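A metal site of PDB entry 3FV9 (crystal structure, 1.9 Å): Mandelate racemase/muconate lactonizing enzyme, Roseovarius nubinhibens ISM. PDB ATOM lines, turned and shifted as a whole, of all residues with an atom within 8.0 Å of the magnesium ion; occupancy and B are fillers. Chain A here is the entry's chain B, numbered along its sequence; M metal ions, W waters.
The backbone NH (N) of Ala 201 lies within hydrogen-bond range of the backbone carbonyl oxygen (O) of Glu 226 (3.1 Å).
The backbone carbonyl oxygen (O) of Ala 199 is in hydrogen-bond range of the backbone NH (N) of Glu 226 (2.8 Å).
The side-chain carboxylate (OD2) of Asp 200 lies close to the side-chain amino group (NZ) of Lys 167.
OD1 of Asp 249 is in salt-bridge range of NZ of Lys 273 (3.3 Å).
The side-chain carboxylate (OE2) of Glu 250 sits at hydrogen-bond distance from the side-chain amide nitrogen (ND2) of Asn 202, 3.3 Å away.
OD1 of Asp 200 is in hydrogen-bond range of N of Asn 202.
NZ of Lys 276 is in salt-bridge range of OD1 of Asp 249.
The side-chain carboxylate of Asp 249 is in hydrogen-bond range of the side-chain hydroxyl of Tyr 59 (3.0 Å).
Water W1 lies within hydrogen-bond range of OD1 of Asp 200 (2.6 Å), OE1 of Glu 250 (2.7 Å) and ND2 of Asn 202 (3.2 Å).
Water W1 binds the magnesium ion, at 2.0 Å.
OE2 of Glu 226 binds the magnesium ion, 2.0 Å away.
Water W3 binds the magnesium ion.
The magnesium ion is bound by OD2 of Asp 200.
Water W2 is bound to the magnesium ion (2.2 Å).
The side-chain carboxylate (OD2) of Asp 249 binds the magnesium ion (2.2 Å).
Residues that only touch the magnesium ion: Asn 202 (3.99 Å).
The nearest printed residue that does not touch the magnesium ion is Lys 273 (4.004 Å).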
ATOM      1  N   TYR A  59      26.902   8.941 -30.870  1.00  0.00           N
ATOM      2  CA  TYR A  59      27.182   8.734 -29.461  1.00  0.00           C
ATOM      3  C   TYR A  59      26.763   9.970 -28.654  1.00  0.00           C
ATOM      4  O   TYR A  59      25.910   9.888 -27.769  1.00  0.00           O
ATOM      5  CB  TYR A  59      28.658   8.375 -29.251  1.00  0.00           C
ATOM      6  CG  TYR A  59      29.084   8.402 -27.807  1.00  0.00           C
ATOM      7  CD1 TYR A  59      28.471   7.568 -26.851  1.00  0.00           C
ATOM      8  CD2 TYR A  59      30.104   9.254 -27.380  1.00  0.00           C
ATOM      9  CE1 TYR A  59      28.855   7.609 -25.517  1.00  0.00           C
ATOM     10  CE2 TYR A  59      30.504   9.289 -26.048  1.00  0.00           C
ATOM     11  CZ  TYR A  59      29.873   8.469 -25.127  1.00  0.00           C
ATOM     12  OH  TYR A  59      30.260   8.510 -23.815  1.00  0.00           O
ATOM     13  N   SER A 165      32.524  -3.674 -18.766  1.00  0.00           N
ATOM     14  CA  SER A 165      31.423  -2.860 -19.261  1.00  0.00           C
ATOM     15  C   SER A 165      30.620  -3.703 -20.229  1.00  0.00           C
ATOM     16  O   SER A 165      31.158  -4.169 -21.242  1.00  0.00           O
ATOM     17  CB  SER A 165      31.955  -1.607 -19.965  1.00  0.00           C
ATOM     18  OG  SER A 165      30.906  -0.731 -20.325  1.00  0.00           O
ATOM     19  N   LYS A 167      27.165  -4.202 -22.705  1.00  0.00           N
ATOM     20  CA  LYS A 167      26.170  -3.419 -23.470  1.00  0.00           C
ATOM     21  C   LYS A 167      24.784  -4.041 -23.383  1.00  0.00           C
ATOM     22  O   LYS A 167      24.615  -5.251 -23.613  1.00  0.00           O
ATOM     23  CB  LYS A 167      26.603  -3.207 -24.940  1.00  0.00           C
ATOM     24  CG  LYS A 167      28.025  -2.667 -25.156  1.00  0.00           C
ATOM     25  CD  LYS A 167      28.362  -1.390 -24.342  1.00  0.00           C
ATOM     26  CE  LYS A 167      29.880  -1.267 -24.177  1.00  0.00           C
ATOM     27  NZ  LYS A 167      30.318  -0.271 -23.121  1.00  0.00           N
ATOM     28  N   LEU A 198      29.535  -2.951 -15.050  1.00  0.00           N
ATOM     29  CA  LEU A 198      28.768  -1.793 -15.486  1.00  0.00           C
ATOM     30  C   LEU A 198      27.875  -2.226 -16.639  1.00  0.00           C
ATOM     31  O   LEU A 198      28.387  -2.669 -17.679  1.00  0.00           O
ATOM     32  CB  LEU A 198      29.697  -0.713 -16.042  1.00  0.00           C
ATOM     33  CG  LEU A 198      30.009   0.648 -15.428  1.00  0.00           C
ATOM     34  CD1 LEU A 198      30.903   1.436 -16.396  1.00  0.00           C
ATOM     35  CD2 LEU A 198      28.754   1.425 -15.081  1.00  0.00           C
ATOM     36  N   ALA A 199      26.561  -2.104 -16.479  1.00  0.00           N
ATOM     37  CA  ALA A 199      25.663  -2.350 -17.594  1.00  0.00           C
ATOM     38  C   ALA A 199      25.388  -1.015 -18.278  1.00  0.00           C
ATOM     39  O   ALA A 199      24.741  -0.127 -17.702  1.00  0.00           O
ATOM     40  CB  ALA A 199      24.392  -3.034 -17.138  1.00  0.00           C
ATOM     41  N   ASP A 200      25.901  -0.861 -19.497  1.00  0.00           N
ATOM     42  CA  ASP A 200      25.824   0.395 -20.239  1.00  0.00           C
ATOM     43  C   ASP A 200      24.749   0.376 -21.315  1.00  0.00           C
ATOM     44  O   ASP A 200      24.861  -0.347 -22.308  1.00  0.00           O
ATOM     45  CB  ASP A 200      27.199   0.736 -20.829  1.00  0.00           C
ATOM     46  CG  ASP A 200      27.251   2.146 -21.423  1.00  0.00           C
ATOM     47  OD1 ASP A 200      26.212   2.811 -21.581  1.00  0.00           O
ATOM     48  OD2 ASP A 200      28.370   2.607 -21.725  1.00  0.00           O
ATOM     49  N   ALA A 201      23.691   1.182 -21.124  1.00  0.00           N
ATOM     50  CA  ALA A 201      22.563   1.231 -22.061  1.00  0.00           C
ATOM     51  C   ALA A 201      22.728   2.278 -23.144  1.00  0.00           C
ATOM     52  O   ALA A 201      21.838   2.431 -23.999  1.00  0.00           O
ATOM     53  CB  ALA A 201      21.247   1.450 -21.317  1.00  0.00           C
ATOM     54  N   ASN A 202      23.842   3.005 -23.111  1.00  0.00           N
ATOM     55  CA  ASN A 202      24.099   4.103 -24.058  1.00  0.00           C
ATOM     56  C   ASN A 202      22.913   5.025 -24.310  1.00  0.00           C
ATOM     57  O   ASN A 202      22.537   5.318 -25.450  1.00  0.00           O
ATOM     58  CB  ASN A 202      24.678   3.566 -25.375  1.00  0.00           C
ATOM     59  CG  ASN A 202      26.139   3.210 -25.234  1.00  0.00           C
ATOM     60  OD1 ASN A 202      26.487   2.038 -25.218  1.00  0.00           O
ATOM     61  ND2 ASN A 202      27.008   4.225 -25.093  1.00  0.00           N
ATOM     62  N   ASN A 203      22.313   5.493 -23.206  1.00  0.00           N
ATOM     63  CA  ASN A 203      21.224   6.480 -23.281  1.00  0.00           C
ATOM     64  C   ASN A 203      20.025   5.955 -24.057  1.00  0.00           C
ATOM     65  O   ASN A 203      19.244   6.730 -24.623  1.00  0.00           O
ATOM     66  CB  ASN A 203      21.748   7.777 -23.901  1.00  0.00           C
ATOM     67  CG  ASN A 203      22.172   8.820 -22.862  1.00  0.00           C
ATOM     68  OD1 ASN A 203      22.030  10.019 -23.100  1.00  0.00           O
ATOM     69  ND2 ASN A 203      22.658   8.369 -21.726  1.00  0.00           N
ATOM     70  N   GLU A 226      24.742   2.196 -16.141  1.00  0.00           N
ATOM     71  CA  GLU A 226      25.288   3.369 -16.831  1.00  0.00           C
ATOM     72  C   GLU A 226      24.339   3.906 -17.926  1.00  0.00           C
ATOM     73  O   GLU A 226      23.796   3.127 -18.718  1.00  0.00           O
ATOM     74  CB  GLU A 226      26.683   3.065 -17.436  1.00  0.00           C
ATOM     75  CG  GLU A 226      27.225   4.128 -18.403  1.00  0.00           C
ATOM     76  CD  GLU A 226      28.644   3.846 -18.906  1.00  0.00           C
ATOM     77  OE1 GLU A 226      29.228   2.782 -18.569  1.00  0.00           O
ATOM     78  OE2 GLU A 226      29.179   4.683 -19.660  1.00  0.00           O
ATOM     79  N   ALA A 227      24.169   5.224 -17.955  1.00  0.00           N
ATOM     80  CA  ALA A 227      23.503   5.901 -19.067  1.00  0.00           C
ATOM     81  C   ALA A 227      22.182   5.205 -19.448  1.00  0.00           C
ATOM     82  O   ALA A 227      22.031   4.728 -20.576  1.00  0.00           O
ATOM     83  CB  ALA A 227      24.455   5.988 -20.282  1.00  0.00           C
ATOM     84  N   LEU A 247      25.332   5.529 -13.041  1.00  0.00           N
ATOM     85  CA  LEU A 247      26.481   6.282 -13.582  1.00  0.00           C
ATOM     86  C   LEU A 247      26.082   7.004 -14.850  1.00  0.00           C
ATOM     87  O   LEU A 247      25.548   6.384 -15.777  1.00  0.00           O
ATOM     88  CB  LEU A 247      27.644   5.322 -13.864  1.00  0.00           C
ATOM     89  CG  LEU A 247      29.005   5.887 -14.273  1.00  0.00           C
ATOM     90  CD1 LEU A 247      30.118   5.075 -13.613  1.00  0.00           C
ATOM     91  CD2 LEU A 247      29.201   5.894 -15.786  1.00  0.00           C
ATOM     92  N   LEU A 248      26.345   8.302 -14.922  1.00  0.00           N
ATOM     93  CA  LEU A 248      25.979   9.047 -16.119  1.00  0.00           C
ATOM     94  C   LEU A 248      27.160   9.268 -17.051  1.00  0.00           C
ATOM     95  O   LEU A 248      28.284   9.497 -16.606  1.00  0.00           O
ATOM     96  CB  LEU A 248      25.297  10.366 -15.763  1.00  0.00           C
ATOM     97  CG  LEU A 248      24.031  10.170 -14.920  1.00  0.00           C
ATOM     98  CD1 LEU A 248      23.412  11.512 -14.629  1.00  0.00           C
ATOM     99  CD2 LEU A 248      23.002   9.209 -15.579  1.00  0.00           C
ATOM    100  N   ASP A 249      26.913   9.180 -18.348  1.00  0.00           N
ATOM    101  CA  ASP A 249      27.992   9.260 -19.325  1.00  0.00           C
ATOM    102  C   ASP A 249      27.696  10.363 -20.357  1.00  0.00           C
ATOM    103  O   ASP A 249      28.171  11.499 -20.198  1.00  0.00           O
ATOM    104  CB  ASP A 249      28.204   7.890 -19.993  1.00  0.00           C
ATOM    105  CG  ASP A 249      29.480   7.820 -20.832  1.00  0.00           C
ATOM    106  OD1 ASP A 249      30.244   8.800 -20.848  1.00  0.00           O
ATOM    107  OD2 ASP A 249      29.738   6.781 -21.486  1.00  0.00           O
ATOM    108  N   GLU A 250      26.896  10.033 -21.380  1.00  0.00           N
ATOM    109  CA  GLU A 250      26.442  11.005 -22.397  1.00  0.00           C
ATOM    110  C   GLU A 250      25.943  12.341 -21.824  1.00  0.00           C
ATOM    111  O   GLU A 250      26.296  13.417 -22.337  1.00  0.00           O
ATOM    112  CB  GLU A 250      25.322  10.411 -23.259  1.00  0.00           C
ATOM    113  CG  GLU A 250      25.771   9.414 -24.322  1.00  0.00           C
ATOM    114  CD  GLU A 250      25.810   7.969 -23.828  1.00  0.00           C
ATOM    115  OE1 GLU A 250      26.187   7.730 -22.658  1.00  0.00           O
ATOM    116  OE2 GLU A 250      25.466   7.052 -24.635  1.00  0.00           O
ATOM    117  N   GLY A 271      30.933   8.667 -16.131  1.00  0.00           N
ATOM    118  CA  GLY A 271      31.834   8.174 -17.173  1.00  0.00           C
ATOM    119  C   GLY A 271      32.519   9.400 -17.743  1.00  0.00           C
ATOM    120  O   GLY A 271      31.900  10.161 -18.504  1.00  0.00           O
ATOM    121  N   LYS A 273      35.037  10.949 -20.188  1.00  0.00           N
ATOM    122  CA  LYS A 273      35.777  10.632 -21.414  1.00  0.00           C
ATOM    123  C   LYS A 273      36.538  11.852 -21.874  1.00  0.00           C
ATOM    124  O   LYS A 273      35.955  12.903 -22.080  1.00  0.00           O
ATOM    125  CB  LYS A 273      34.846  10.112 -22.493  1.00  0.00           C
ATOM    126  CG  LYS A 273      34.381   8.676 -22.195  1.00  0.00           C
ATOM    127  CD  LYS A 273      33.461   8.160 -23.255  1.00  0.00           C
ATOM    128  CE  LYS A 273      32.949   6.746 -22.915  1.00  0.00           C
ATOM    129  NZ  LYS A 273      32.556   6.603 -21.495  1.00  0.00           N
ATOM    130  N   LYS A 276      35.098  13.924 -24.733  1.00  0.00           N
ATOM    131  CA  LYS A 276      33.733  14.333 -24.398  1.00  0.00           C
ATOM    132  C   LYS A 276      33.742  15.519 -23.413  1.00  0.00           C
ATOM    133  O   LYS A 276      32.990  16.479 -23.606  1.00  0.00           O
ATOM    134  CB  LYS A 276      32.902  13.154 -23.835  1.00  0.00           C
ATOM    135  CG  LYS A 276      31.548  13.572 -23.228  1.00  0.00           C
ATOM    136  CD  LYS A 276      30.545  12.409 -23.076  1.00  0.00           C
ATOM    137  CE  LYS A 276      30.981  11.338 -22.081  1.00  0.00           C
ATOM    138  NZ  LYS A 276      30.854  11.746 -20.625  1.00  0.00           N
ATOM    139  N   GLN A 300      37.971   7.263 -19.317  1.00  0.00           N
ATOM    140  CA  GLN A 300      37.954   6.663 -20.646  1.00  0.00           C
ATOM    141  C   GLN A 300      38.131   7.722 -21.732  1.00  0.00           C
ATOM    142  O   GLN A 300      38.485   8.868 -21.436  1.00  0.00           O
ATOM    143  CB  GLN A 300      36.628   5.904 -20.844  1.00  0.00           C
ATOM    144  CG  GLN A 300      36.354   4.819 -19.788  1.00  0.00           C
ATOM    145  CD  GLN A 300      35.156   3.949 -20.129  1.00  0.00           C
ATOM    146  OE1 GLN A 300      34.680   3.949 -21.255  1.00  0.00           O
ATOM    147  NE2 GLN A 300      34.656   3.206 -19.139  1.00  0.00           N
HETATM  148 MG    MG M   1      29.054   4.673 -21.697  1.00  0.00          MG
HETATM  149  O   HOH W   1      27.147   5.227 -22.050  1.00  0.00           O
HETATM  150  O   HOH W   2      31.126   4.001 -21.572  1.00  0.00           O
HETATM  151  O   HOH W   3      29.410   4.561 -23.777  1.00  0.00           O
